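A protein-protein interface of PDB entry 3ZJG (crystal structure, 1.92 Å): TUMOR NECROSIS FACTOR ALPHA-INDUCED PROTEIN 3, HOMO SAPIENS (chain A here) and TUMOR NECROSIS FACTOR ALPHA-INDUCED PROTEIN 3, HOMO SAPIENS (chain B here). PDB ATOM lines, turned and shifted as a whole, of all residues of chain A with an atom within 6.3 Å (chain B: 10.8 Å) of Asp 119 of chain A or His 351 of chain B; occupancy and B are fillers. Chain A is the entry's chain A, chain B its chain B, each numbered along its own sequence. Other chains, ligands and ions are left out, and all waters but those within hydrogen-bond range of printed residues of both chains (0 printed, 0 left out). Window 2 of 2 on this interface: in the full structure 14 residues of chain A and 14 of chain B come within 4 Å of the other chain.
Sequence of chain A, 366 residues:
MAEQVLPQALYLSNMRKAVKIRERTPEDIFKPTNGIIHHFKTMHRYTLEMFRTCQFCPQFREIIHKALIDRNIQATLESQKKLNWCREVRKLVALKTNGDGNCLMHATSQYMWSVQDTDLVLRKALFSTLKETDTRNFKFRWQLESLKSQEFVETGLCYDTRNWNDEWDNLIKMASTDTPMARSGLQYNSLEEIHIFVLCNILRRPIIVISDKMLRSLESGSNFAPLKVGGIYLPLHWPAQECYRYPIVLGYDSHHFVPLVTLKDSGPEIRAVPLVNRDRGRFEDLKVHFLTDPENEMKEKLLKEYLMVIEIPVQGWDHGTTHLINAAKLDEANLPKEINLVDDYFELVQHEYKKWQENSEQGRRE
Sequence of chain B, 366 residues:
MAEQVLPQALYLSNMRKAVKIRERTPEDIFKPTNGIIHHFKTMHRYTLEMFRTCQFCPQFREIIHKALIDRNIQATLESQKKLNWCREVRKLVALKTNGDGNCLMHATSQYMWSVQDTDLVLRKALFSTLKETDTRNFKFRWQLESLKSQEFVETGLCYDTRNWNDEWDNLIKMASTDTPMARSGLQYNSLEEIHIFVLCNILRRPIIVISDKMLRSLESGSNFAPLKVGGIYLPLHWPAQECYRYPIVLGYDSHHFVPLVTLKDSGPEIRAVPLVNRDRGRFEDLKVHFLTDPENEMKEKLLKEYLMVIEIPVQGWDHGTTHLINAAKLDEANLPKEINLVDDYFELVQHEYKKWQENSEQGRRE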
ATOM      1  N   VAL A  19     -12.848  19.853 -29.525  1.00  0.00           N
ATOM      2  CA  VAL A  19     -12.382  19.266 -28.296  1.00  0.00           C
ATOM      3  C   VAL A  19     -11.663  20.250 -27.360  1.00  0.00           C
ATOM      4  O   VAL A  19     -11.902  20.224 -26.160  1.00  0.00           O
ATOM      5  CB  VAL A  19     -11.488  18.021 -28.577  1.00  0.00           C
ATOM      6  CG1 VAL A  19     -10.584  17.716 -27.379  1.00  0.00           C
ATOM      7  CG2 VAL A  19     -12.381  16.839 -28.926  1.00  0.00           C
ATOM      8  N   ARG A  22     -14.384  22.477 -25.791  1.00  0.00           N
ATOM      9  CA  ARG A  22     -15.033  21.686 -24.759  1.00  0.00           C
ATOM     10  C   ARG A  22     -14.170  21.403 -23.527  1.00  0.00           C
ATOM     11  O   ARG A  22     -14.633  21.607 -22.402  1.00  0.00           O
ATOM     12  CB  ARG A  22     -15.658  20.438 -25.379  1.00  0.00           C
ATOM     13  CG  ARG A  22     -16.729  20.892 -26.422  1.00  0.00           C
ATOM     14  CD  ARG A  22     -17.831  19.899 -26.625  1.00  0.00           C
ATOM     15  NE  ARG A  22     -17.264  18.776 -27.346  1.00  0.00           N
ATOM     16  CZ  ARG A  22     -17.303  18.640 -28.670  1.00  0.00           C
ATOM     17  NH1 ARG A  22     -17.964  19.526 -29.427  1.00  0.00           N
ATOM     18  NH2 ARG A  22     -16.715  17.583 -29.236  1.00  0.00           N
ATOM     19  N   GLU A  23     -12.922  21.002 -23.711  1.00  0.00           N
ATOM     20  CA  GLU A  23     -12.033  20.783 -22.561  1.00  0.00           C
ATOM     21  C   GLU A  23     -11.824  22.043 -21.685  1.00  0.00           C
ATOM     22  O   GLU A  23     -11.442  21.953 -20.526  1.00  0.00           O
ATOM     23  CB  GLU A  23     -10.688  20.292 -23.029  1.00  0.00           C
ATOM     24  CG  GLU A  23     -10.661  18.819 -23.370  1.00  0.00           C
ATOM     25  CD  GLU A  23      -9.257  18.315 -23.535  1.00  0.00           C
ATOM     26  OE1 GLU A  23      -8.322  19.145 -23.506  1.00  0.00           O
ATOM     27  OE2 GLU A  23      -9.084  17.094 -23.685  1.00  0.00           O
ATOM     28  N   THR A  25     -14.311  24.294 -20.918  1.00  0.00           N
ATOM     29  CA  THR A  25     -15.552  24.588 -20.229  1.00  0.00           C
ATOM     30  C   THR A  25     -15.639  24.114 -18.762  1.00  0.00           C
ATOM     31  O   THR A  25     -15.914  24.952 -17.912  1.00  0.00           O
ATOM     32  CB  THR A  25     -16.797  24.154 -21.084  1.00  0.00           C
ATOM     33  OG1 THR A  25     -16.699  22.768 -21.398  1.00  0.00           O
ATOM     34  CG2 THR A  25     -16.844  24.937 -22.407  1.00  0.00           C
ATOM     35  N   GLN A 116     -21.365  21.988 -29.696  1.00  0.00           N
ATOM     36  CA  GLN A 116     -22.527  21.502 -28.956  1.00  0.00           C
ATOM     37  C   GLN A 116     -22.057  20.914 -27.622  1.00  0.00           C
ATOM     38  O   GLN A 116     -20.843  20.884 -27.357  1.00  0.00           O
ATOM     39  CB  GLN A 116     -23.330  20.491 -29.840  1.00  0.00           C
ATOM     40  CG  GLN A 116     -23.983  21.261 -31.062  1.00  0.00           C
ATOM     41  CD  GLN A 116     -24.888  20.422 -32.006  1.00  0.00           C
ATOM     42  OE1 GLN A 116     -25.798  19.714 -31.566  1.00  0.00           O
ATOM     43  NE2 GLN A 116     -24.629  20.520 -33.302  1.00  0.00           N
ATOM     44  N   ASP A 117     -23.006  20.471 -26.783  1.00  0.00           N
ATOM     45  CA  ASP A 117     -22.711  19.984 -25.427  1.00  0.00           C
ATOM     46  C   ASP A 117     -22.399  18.493 -25.400  1.00  0.00           C
ATOM     47  O   ASP A 117     -22.933  17.730 -24.603  1.00  0.00           O
ATOM     48  CB  ASP A 117     -23.882  20.329 -24.491  1.00  0.00           C
ATOM     49  CG  ASP A 117     -23.526  20.202 -23.000  1.00  0.00           C
ATOM     50  OD1 ASP A 117     -22.458  20.723 -22.552  1.00  0.00           O
ATOM     51  OD2 ASP A 117     -24.374  19.630 -22.256  1.00  0.00           O
ATOM     52  N   THR A 118     -21.487  18.080 -26.262  1.00  0.00           N
ATOM     53  CA  THR A 118     -21.358  16.657 -26.476  1.00  0.00           C
ATOM     54  C   THR A 118     -20.538  15.987 -25.381  1.00  0.00           C
ATOM     55  O   THR A 118     -20.595  14.782 -25.250  1.00  0.00           O
ATOM     56  CB  THR A 118     -20.810  16.332 -27.882  1.00  0.00           C
ATOM     57  OG1 THR A 118     -19.649  17.119 -28.109  1.00  0.00           O
ATOM     58  CG2 THR A 118     -21.832  16.685 -28.944  1.00  0.00           C
ATOM     59  N   ASP A 119     -19.863  16.772 -24.528  1.00  0.00           N
ATOM     60  CA  ASP A 119     -19.327  16.193 -23.299  1.00  0.00           C
ATOM     61  C   ASP A 119     -20.305  16.276 -22.127  1.00  0.00           C
ATOM     62  O   ASP A 119     -19.946  15.902 -21.025  1.00  0.00           O
ATOM     63  CB  ASP A 119     -17.976  16.831 -22.906  1.00  0.00           C
ATOM     64  CG  ASP A 119     -16.842  16.466 -23.888  1.00  0.00           C
ATOM     65  OD1 ASP A 119     -16.992  15.458 -24.567  1.00  0.00           O
ATOM     66  OD2 ASP A 119     -15.819  17.189 -23.982  1.00  0.00           O
ATOM     67  N   LEU A 120     -21.500  16.824 -22.346  1.00  0.00           N
ATOM     68  CA  LEU A 120     -22.523  16.865 -21.290  1.00  0.00           C
ATOM     69  C   LEU A 120     -22.143  17.806 -20.138  1.00  0.00           C
ATOM     70  O   LEU A 120     -22.639  17.662 -19.013  1.00  0.00           O
ATOM     71  CB  LEU A 120     -22.774  15.458 -20.723  1.00  0.00           C
ATOM     72  CG  LEU A 120     -23.821  14.530 -21.380  1.00  0.00           C
ATOM     73  CD1 LEU A 120     -24.362  15.020 -22.724  1.00  0.00           C
ATOM     74  CD2 LEU A 120     -23.391  13.103 -21.467  1.00  0.00           C
ATOM     75  N   VAL A 121     -21.275  18.771 -20.396  1.00  0.00           N
ATOM     76  CA  VAL A 121     -20.815  19.627 -19.303  1.00  0.00           C
ATOM     77  C   VAL A 121     -21.986  20.472 -18.752  1.00  0.00           C
ATOM     78  O   VAL A 121     -22.208  20.585 -17.520  1.00  0.00           O
ATOM     79  CB  VAL A 121     -19.679  20.504 -19.786  1.00  0.00           C
ATOM     80  CG1 VAL A 121     -19.388  21.584 -18.779  1.00  0.00           C
ATOM     81  CG2 VAL A 121     -18.427  19.638 -20.070  1.00  0.00           C
ATOM     82  N   LEU A 122     -22.758  21.046 -19.664  1.00  0.00           N
ATOM     83  CA  LEU A 122     -23.841  21.915 -19.238  1.00  0.00           C
ATOM     84  C   LEU A 122     -24.936  21.084 -18.588  1.00  0.00           C
ATOM     85  O   LEU A 122     -25.485  21.478 -17.568  1.00  0.00           O
ATOM     86  CB  LEU A 122     -24.381  22.687 -20.426  1.00  0.00           C
ATOM     87  CG  LEU A 122     -23.472  23.860 -20.852  1.00  0.00           C
ATOM     88  CD1 LEU A 122     -24.104  24.604 -22.007  1.00  0.00           C
ATOM     89  CD2 LEU A 122     -23.243  24.847 -19.680  1.00  0.00           C
ATOM     90  N   LYS A 124     -24.739  18.105 -17.073  1.00  0.00           N
ATOM     91  CA  LYS A 124     -24.264  17.739 -15.731  1.00  0.00           C
ATOM     92  C   LYS A 124     -24.313  18.879 -14.698  1.00  0.00           C
ATOM     93  O   LYS A 124     -24.613  18.653 -13.528  1.00  0.00           O
ATOM     94  CB  LYS A 124     -22.848  17.171 -15.820  1.00  0.00           C
ATOM     95  CG  LYS A 124     -22.877  15.743 -16.276  1.00  0.00           C
ATOM     96  CD  LYS A 124     -21.516  15.113 -16.462  1.00  0.00           C
ATOM     97  CE  LYS A 124     -21.728  13.727 -17.074  1.00  0.00           C
ATOM     98  NZ  LYS A 124     -20.495  12.980 -17.495  1.00  0.00           N
ATOM     99  N   VAL B   5     -17.867   8.185 -33.426  1.00  0.00           N
ATOM    100  CA  VAL B   5     -17.536   9.439 -32.742  1.00  0.00           C
ATOM    101  C   VAL B   5     -16.108   9.899 -33.079  1.00  0.00           C
ATOM    102  O   VAL B   5     -15.802  11.095 -33.037  1.00  0.00           O
ATOM    103  CB  VAL B   5     -17.718   9.329 -31.205  1.00  0.00           C
ATOM    104  N   LEU B   6     -15.239   8.946 -33.410  1.00  0.00           N
ATOM    105  CA  LEU B   6     -13.926   9.274 -33.980  1.00  0.00           C
ATOM    106  C   LEU B   6     -14.044   9.791 -35.423  1.00  0.00           C
ATOM    107  O   LEU B   6     -15.128   9.784 -35.998  1.00  0.00           O
ATOM    108  CB  LEU B   6     -12.994   8.066 -33.916  1.00  0.00           C
ATOM    109  CG  LEU B   6     -12.423   7.808 -32.521  1.00  0.00           C
ATOM    110  CD1 LEU B   6     -11.465   6.629 -32.528  1.00  0.00           C
ATOM    111  CD2 LEU B   6     -11.712   9.037 -32.000  1.00  0.00           C
ATOM    112  N   PRO B   7     -12.941  10.287 -36.002  1.00  0.00           N
ATOM    113  CA  PRO B   7     -13.068  10.639 -37.418  1.00  0.00           C
ATOM    114  C   PRO B   7     -12.909   9.433 -38.345  1.00  0.00           C
ATOM    115  O   PRO B   7     -11.886   8.729 -38.330  1.00  0.00           O
ATOM    116  CB  PRO B   7     -11.943  11.660 -37.636  1.00  0.00           C
ATOM    117  CG  PRO B   7     -11.635  12.167 -36.265  1.00  0.00           C
ATOM    118  CD  PRO B   7     -11.804  10.976 -35.379  1.00  0.00           C
ATOM    119  N   PHE B  51       0.847   6.611 -34.903  1.00  0.00           N
ATOM    120  CA  PHE B  51       0.912   6.428 -33.453  1.00  0.00           C
ATOM    121  C   PHE B  51       0.532   5.014 -33.091  1.00  0.00           C
ATOM    122  O   PHE B  51      -0.207   4.332 -33.827  1.00  0.00           O
ATOM    123  CB  PHE B  51       0.041   7.446 -32.692  1.00  0.00           C
ATOM    124  CG  PHE B  51      -1.424   7.409 -33.058  1.00  0.00           C
ATOM    125  CD1 PHE B  51      -2.272   6.462 -32.488  1.00  0.00           C
ATOM    126  CD2 PHE B  51      -1.955   8.345 -33.962  1.00  0.00           C
ATOM    127  CE1 PHE B  51      -3.621   6.415 -32.823  1.00  0.00           C
ATOM    128  CE2 PHE B  51      -3.321   8.323 -34.318  1.00  0.00           C
ATOM    129  CZ  PHE B  51      -4.159   7.363 -33.739  1.00  0.00           C
ATOM    130  N   PHE B  56      -4.408   0.989 -26.091  1.00  0.00           N
ATOM    131  CA  PHE B  56      -5.867   1.071 -26.073  1.00  0.00           C
ATOM    132  C   PHE B  56      -6.522  -0.325 -25.931  1.00  0.00           C
ATOM    133  O   PHE B  56      -5.825  -1.339 -25.838  1.00  0.00           O
ATOM    134  CB  PHE B  56      -6.369   1.894 -27.273  1.00  0.00           C
ATOM    135  CG  PHE B  56      -5.829   3.314 -27.277  1.00  0.00           C
ATOM    136  CD1 PHE B  56      -6.265   4.232 -26.317  1.00  0.00           C
ATOM    137  CD2 PHE B  56      -4.872   3.720 -28.207  1.00  0.00           C
ATOM    138  CE1 PHE B  56      -5.761   5.529 -26.283  1.00  0.00           C
ATOM    139  CE2 PHE B  56      -4.358   5.018 -28.179  1.00  0.00           C
ATOM    140  CZ  PHE B  56      -4.812   5.929 -27.208  1.00  0.00           C
ATOM    141  N   PHE B  60     -11.806  -0.348 -29.301  1.00  0.00           N
ATOM    142  CA  PHE B  60     -11.274   0.993 -29.540  1.00  0.00           C
ATOM    143  C   PHE B  60     -10.250   0.917 -30.703  1.00  0.00           C
ATOM    144  O   PHE B  60     -10.367   1.645 -31.695  1.00  0.00           O
ATOM    145  CB  PHE B  60     -10.618   1.472 -28.223  1.00  0.00           C
ATOM    146  CG  PHE B  60     -10.518   2.965 -28.065  1.00  0.00           C
ATOM    147  CD1 PHE B  60     -11.626   3.710 -27.697  1.00  0.00           C
ATOM    148  CD2 PHE B  60      -9.300   3.610 -28.233  1.00  0.00           C
ATOM    149  CE1 PHE B  60     -11.538   5.074 -27.532  1.00  0.00           C
ATOM    150  CE2 PHE B  60      -9.200   4.975 -28.077  1.00  0.00           C
ATOM    151  CZ  PHE B  60     -10.328   5.709 -27.724  1.00  0.00           C
ATOM    152  N   ILE B  64     -10.104   2.631 -34.489  1.00  0.00           N
ATOM    153  CA  ILE B  64      -8.968   3.351 -35.038  1.00  0.00           C
ATOM    154  C   ILE B  64      -8.500   2.685 -36.338  1.00  0.00           C
ATOM    155  O   ILE B  64      -8.369   3.359 -37.404  1.00  0.00           O
ATOM    156  CB  ILE B  64      -7.791   3.429 -34.010  1.00  0.00           C
ATOM    157  CG1 ILE B  64      -8.307   4.039 -32.684  1.00  0.00           C
ATOM    158  CG2 ILE B  64      -6.656   4.221 -34.602  1.00  0.00           C
ATOM    159  CD1 ILE B  64      -7.296   4.125 -31.520  1.00  0.00           C
ATOM    160  N   VAL B 342      -2.084  13.687 -38.130  1.00  0.00           N
ATOM    161  CA  VAL B 342      -1.969  12.581 -37.202  1.00  0.00           C
ATOM    162  C   VAL B 342      -1.903  12.985 -35.696  1.00  0.00           C
ATOM    163  O   VAL B 342      -2.644  12.408 -34.878  1.00  0.00           O
ATOM    164  CB  VAL B 342      -0.789  11.635 -37.661  1.00  0.00           C
ATOM    165  CG1 VAL B 342      -0.420  10.683 -36.547  1.00  0.00           C
ATOM    166  CG2 VAL B 342      -1.190  10.859 -38.953  1.00  0.00           C
ATOM    167  N   ASP B 343      -1.110  14.005 -35.325  1.00  0.00           N
ATOM    168  CA  ASP B 343      -1.113  14.491 -33.925  1.00  0.00           C
ATOM    169  C   ASP B 343      -2.489  14.972 -33.469  1.00  0.00           C
ATOM    170  O   ASP B 343      -2.900  14.726 -32.327  1.00  0.00           O
ATOM    171  CB  ASP B 343      -0.071  15.607 -33.688  1.00  0.00           C
ATOM    172  CG  ASP B 343       1.367  15.133 -33.943  1.00  0.00           C
ATOM    173  OD1 ASP B 343       1.758  14.054 -33.404  1.00  0.00           O
ATOM    174  OD2 ASP B 343       2.093  15.831 -34.702  1.00  0.00           O
ATOM    175  N   ASP B 344      -3.208  15.672 -34.343  1.00  0.00           N
ATOM    176  CA  ASP B 344      -4.553  16.074 -33.981  1.00  0.00           C
ATOM    177  C   ASP B 344      -5.439  14.858 -33.838  1.00  0.00           C
ATOM    178  O   ASP B 344      -6.242  14.802 -32.906  1.00  0.00           O
ATOM    179  CB  ASP B 344      -5.179  17.069 -34.984  1.00  0.00           C
ATOM    180  CG  ASP B 344      -4.572  18.446 -34.909  1.00  0.00           C
ATOM    181  OD1 ASP B 344      -4.273  18.930 -33.801  1.00  0.00           O
ATOM    182  OD2 ASP B 344      -4.401  19.066 -35.973  1.00  0.00           O
ATOM    183  N   TYR B 345      -5.346  13.910 -34.772  1.00  0.00           N
ATOM    184  CA  TYR B 345      -6.077  12.636 -34.645  1.00  0.00           C
ATOM    185  C   TYR B 345      -5.803  12.008 -33.290  1.00  0.00           C
ATOM    186  O   TYR B 345      -6.723  11.568 -32.589  1.00  0.00           O
ATOM    187  CB  TYR B 345      -5.683  11.605 -35.718  1.00  0.00           C
ATOM    188  CG  TYR B 345      -6.787  10.603 -35.919  1.00  0.00           C
ATOM    189  CD1 TYR B 345      -6.891   9.493 -35.112  1.00  0.00           C
ATOM    190  CD2 TYR B 345      -7.765  10.812 -36.880  1.00  0.00           C
ATOM    191  CE1 TYR B 345      -7.913   8.599 -35.253  1.00  0.00           C
ATOM    192  CE2 TYR B 345      -8.806   9.901 -37.039  1.00  0.00           C
ATOM    193  CZ  TYR B 345      -8.867   8.792 -36.209  1.00  0.00           C
ATOM    194  OH  TYR B 345      -9.899   7.886 -36.328  1.00  0.00           O
ATOM    195  N   PHE B 346      -4.528  11.984 -32.917  1.00  0.00           N
ATOM    196  CA  PHE B 346      -4.126  11.391 -31.647  1.00  0.00           C
ATOM    197  C   PHE B 346      -4.777  12.055 -30.426  1.00  0.00           C
ATOM    198  O   PHE B 346      -5.279  11.359 -29.514  1.00  0.00           O
ATOM    199  CB  PHE B 346      -2.597  11.349 -31.512  1.00  0.00           C
ATOM    200  CG  PHE B 346      -2.139  10.679 -30.264  1.00  0.00           C
ATOM    201  CD1 PHE B 346      -2.083   9.305 -30.189  1.00  0.00           C
ATOM    202  CD2 PHE B 346      -1.841  11.431 -29.132  1.00  0.00           C
ATOM    203  CE1 PHE B 346      -1.686   8.676 -29.015  1.00  0.00           C
ATOM    204  CE2 PHE B 346      -1.449  10.818 -27.965  1.00  0.00           C
ATOM    205  CZ  PHE B 346      -1.368   9.440 -27.909  1.00  0.00           C
ATOM    206  N   GLU B 347      -4.774  13.381 -30.385  1.00  0.00           N
ATOM    207  CA  GLU B 347      -5.435  14.057 -29.253  1.00  0.00           C
ATOM    208  C   GLU B 347      -6.916  13.819 -29.236  1.00  0.00           C
ATOM    209  O   GLU B 347      -7.510  13.681 -28.150  1.00  0.00           O
ATOM    210  CB  GLU B 347      -5.140  15.544 -29.205  1.00  0.00           C
ATOM    211  CG  GLU B 347      -3.952  15.882 -28.321  1.00  0.00           C
ATOM    212  CD  GLU B 347      -2.903  16.715 -29.041  1.00  0.00           C
ATOM    213  OE1 GLU B 347      -3.240  17.815 -29.534  1.00  0.00           O
ATOM    214  OE2 GLU B 347      -1.739  16.272 -29.110  1.00  0.00           O
ATOM    215  N   LEU B 348      -7.537  13.800 -30.410  1.00  0.00           N
ATOM    216  CA  LEU B 348      -8.937  13.382 -30.494  1.00  0.00           C
ATOM    217  C   LEU B 348      -9.094  12.030 -29.808  1.00  0.00           C
ATOM    218  O   LEU B 348      -9.929  11.864 -28.926  1.00  0.00           O
ATOM    219  CB  LEU B 348      -9.446  13.323 -31.933  1.00  0.00           C
ATOM    220  CG  LEU B 348      -9.794  14.672 -32.579  1.00  0.00           C
ATOM    221  CD1 LEU B 348     -10.447  14.496 -33.919  1.00  0.00           C
ATOM    222  CD2 LEU B 348     -10.701  15.502 -31.672  1.00  0.00           C
ATOM    223  N   VAL B 349      -8.233  11.080 -30.187  1.00  0.00           N
ATOM    224  CA  VAL B 349      -8.238   9.753 -29.584  1.00  0.00           C
ATOM    225  C   VAL B 349      -8.057   9.749 -28.060  1.00  0.00           C
ATOM    226  O   VAL B 349      -8.840   9.123 -27.355  1.00  0.00           O
ATOM    227  CB  VAL B 349      -7.201   8.813 -30.266  1.00  0.00           C
ATOM    228  CG1 VAL B 349      -6.990   7.550 -29.446  1.00  0.00           C
ATOM    229  CG2 VAL B 349      -7.661   8.448 -31.652  1.00  0.00           C
ATOM    230  N   GLN B 350      -7.052  10.460 -27.564  1.00  0.00           N
ATOM    231  CA  GLN B 350      -6.838  10.580 -26.126  1.00  0.00           C
ATOM    232  C   GLN B 350      -8.019  11.186 -25.384  1.00  0.00           C
ATOM    233  O   GLN B 350      -8.346  10.717 -24.310  1.00  0.00           O
ATOM    234  CB  GLN B 350      -5.575  11.359 -25.804  1.00  0.00           C
ATOM    235  CG  GLN B 350      -4.320  10.478 -25.807  1.00  0.00           C
ATOM    236  CD  GLN B 350      -3.151  11.162 -25.150  1.00  0.00           C
ATOM    237  OE1 GLN B 350      -3.133  12.389 -25.028  1.00  0.00           O
ATOM    238  NE2 GLN B 350      -2.167  10.379 -24.719  1.00  0.00           N
ATOM    239  N   HIS B 351      -8.645  12.228 -25.942  1.00  0.00           N
ATOM    240  CA  HIS B 351      -9.819  12.844 -25.280  1.00  0.00           C
ATOM    241  C   HIS B 351     -10.939  11.823 -25.230  1.00  0.00           C
ATOM    242  O   HIS B 351     -11.590  11.666 -24.232  1.00  0.00           O
ATOM    243  CB  HIS B 351     -10.300  14.112 -25.998  1.00  0.00           C
ATOM    244  CG  HIS B 351     -11.520  14.727 -25.369  1.00  0.00           C
ATOM    245  ND1 HIS B 351     -11.453  15.725 -24.415  1.00  0.00           N
ATOM    246  CD2 HIS B 351     -12.841  14.473 -25.547  1.00  0.00           C
ATOM    247  CE1 HIS B 351     -12.675  16.047 -24.030  1.00  0.00           C
ATOM    248  NE2 HIS B 351     -13.536  15.300 -24.695  1.00  0.00           N
ATOM    249  N   GLU B 352     -11.132  11.095 -26.323  1.00  0.00           N
ATOM    250  CA  GLU B 352     -12.187  10.085 -26.377  1.00  0.00           C
ATOM    251  C   GLU B 352     -11.924   8.858 -25.485  1.00  0.00           C
ATOM    252  O   GLU B 352     -12.833   8.358 -24.812  1.00  0.00           O
ATOM    253  CB  GLU B 352     -12.444   9.667 -27.827  1.00  0.00           C
ATOM    254  CG  GLU B 352     -13.123  10.749 -28.677  1.00  0.00           C
ATOM    255  CD  GLU B 352     -14.412  11.259 -28.065  1.00  0.00           C
ATOM    256  OE1 GLU B 352     -15.357  10.457 -27.840  1.00  0.00           O
ATOM    257  OE2 GLU B 352     -14.475  12.477 -27.799  1.00  0.00           O
ATOM    258  N   TYR B 353     -10.693   8.379 -25.458  1.00  0.00           N
ATOM    259  CA  TYR B 353     -10.372   7.262 -24.578  1.00  0.00           C
ATOM    260  C   TYR B 353     -10.734   7.517 -23.101  1.00  0.00           C
ATOM    261  O   TYR B 353     -11.324   6.645 -22.461  1.00  0.00           O
ATOM    262  CB  TYR B 353      -8.910   6.837 -24.732  1.00  0.00           C
ATOM    263  CG  TYR B 353      -8.623   5.467 -24.142  1.00  0.00           C
ATOM    264  CD1 TYR B 353      -9.355   4.347 -24.546  1.00  0.00           C
ATOM    265  CD2 TYR B 353      -7.623   5.291 -23.182  1.00  0.00           C
ATOM    266  CE1 TYR B 353      -9.102   3.094 -24.001  1.00  0.00           C
ATOM    267  CE2 TYR B 353      -7.366   4.049 -22.635  1.00  0.00           C
ATOM    268  CZ  TYR B 353      -8.105   2.952 -23.051  1.00  0.00           C
ATOM    269  OH  TYR B 353      -7.851   1.700 -22.522  1.00  0.00           O
ATOM    270  N   LYS B 354     -10.429   8.703 -22.568  1.00  0.00           N
ATOM    271  CA  LYS B 354     -10.768   9.007 -21.171  1.00  0.00           C
ATOM    272  C   LYS B 354     -12.256   8.874 -20.885  1.00  0.00           C
ATOM    273  O   LYS B 354     -12.646   8.470 -19.788  1.00  0.00           O
ATOM    274  CB  LYS B 354     -10.288  10.401 -20.745  1.00  0.00           C
ATOM    275  CG  LYS B 354      -8.784  10.558 -20.856  1.00  0.00           C
ATOM    276  N   LYS B 355     -13.086   9.210 -21.869  1.00  0.00           N
ATOM    277  CA  LYS B 355     -14.539   9.072 -21.716  1.00  0.00           C
ATOM    278  C   LYS B 355     -14.913   7.597 -21.670  1.00  0.00           C
ATOM    279  O   LYS B 355     -15.909   7.221 -21.064  1.00  0.00           O
ATOM    280  CB  LYS B 355     -15.292   9.759 -22.867  1.00  0.00           C
ATOM    281  CG  LYS B 355     -15.045  11.266 -22.998  1.00  0.00           C
ATOM    282  CD  LYS B 355     -16.355  12.046 -23.108  1.00  0.00           C
ATOM    283  CE  LYS B 355     -16.979  11.926 -24.495  1.00  0.00           C
ATOM    284  NZ  LYS B 355     -18.297  12.635 -24.549  1.00  0.00           N
ATOM    285  N   TRP B 356     -14.101   6.771 -22.325  1.00  0.00           N
ATOM    286  CA  TRP B 356     -14.309   5.321 -22.395  1.00  0.00           C
ATOM    287  C   TRP B 356     -13.699   4.571 -21.188  1.00  0.00           C
ATOM    288  O   TRP B 356     -13.826   3.350 -21.070  1.00  0.00           O
ATOM    289  CB  TRP B 356     -13.716   4.775 -23.711  1.00  0.00           C
ATOM    290  N   GLN B 357     -13.031   5.306 -20.303  1.00  0.00           N
ATOM    291  CA  GLN B 357     -12.373   4.704 -19.152  1.00  0.00           C
ATOM    292  C   GLN B 357     -13.028   5.182 -17.856  1.00  0.00           C
ATOM    293  O   GLN B 357     -14.075   5.831 -17.882  1.00  0.00           O
ATOM    294  CB  GLN B 357     -10.874   5.027 -19.160  1.00  0.00           C
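The side-chain carboxylate (OE2) of Glu 23 of chain A is in hydrogen-bond range of a ring nitrogen (ND1) of His 351 of chain B (2.8 Å). OD1 of Asp 119 of chain A is in salt-bridge range of NZ of Lys 355 of chain B (3.1 Å). The side-chain amino group (NZ) of Lys 355 of chain B lies within hydrogen-bond range of the backbone carbonyl oxygen (O) of Thr 118 of chain A, 3.2 Å away. OD2 of Asp 119 of chain A lies within hydrogen-bond range of NE2 of His 351 of chain B (3.0 Å).
The guanidinium group of Arg 22 of chain A lies close to the side-chain hydroxyl of Thr 118 of chain A (3.0 Å). The side-chain carboxylate (OD2) of Asp 119 of chain A is in salt-bridge range of the guanidinium group (NE) of Arg 22 of chain A, at 3.99 Å.
Of the printed residues of chain B, Glu 23 of chain A touches His 351 (2.8 Å). No residue of chain B comes within 4 Å of Asp 117 of chain A. Of chain B, only Lys 355 (3.2 Å) comes within 4 Å of Thr 118 of chain A. Of chain B, only His 351 and Lys 355 come within 4 Å of Asp 119 of chain A. No residue of chain B comes within 4 Å of Val 121 of chain A. Of the printed residues of chain A, Leu 348 of chain B touches Val 19. Of chain A, only Val 19 (3.7 Å), Glu 23 (2.8 Å) and Asp 119 (3.0 Å) come within 4 Å of His 351 of chain B. Glu 352 of chain B touches none of the printed residues of chain A. Printed residues of chain A within 4 Å of Lys 355 of chain B: Thr 118 and Asp 119. The nearest residue of chain B that does not touch Asp 119 of chain A is Glu 352 of chain B (5.1 Å). The nearest printed residue of chain A that does not touch Leu 348 of chain B is Arg 22 of chain A (6.8 Å).
Printed residues of chain A that touch a printed residue of chain B: Val 19, Glu 23, Thr 118 and Asp 119. Hydrophobic or aromatic side chains of chain A that line the printed part of chain B: Val 19. Of the 23 printed residues of chain B, 3 touch a printed residue of chain A. Among the printed residues, 6 pairs touch across the chains. Among the printed residues, Asp or Glu carboxylates within 4 Å of a Lys or Arg side-chain nitrogen of the other chain: Asp 119 of chain A with Lys 355 of chain B.
Among the printed residues, merely in contact across the chains: Val 19 of chain A with Leu 348 of chain B (3.5 Å) and Val 19 of chain A with His 351 of chain B (3.7 Å).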
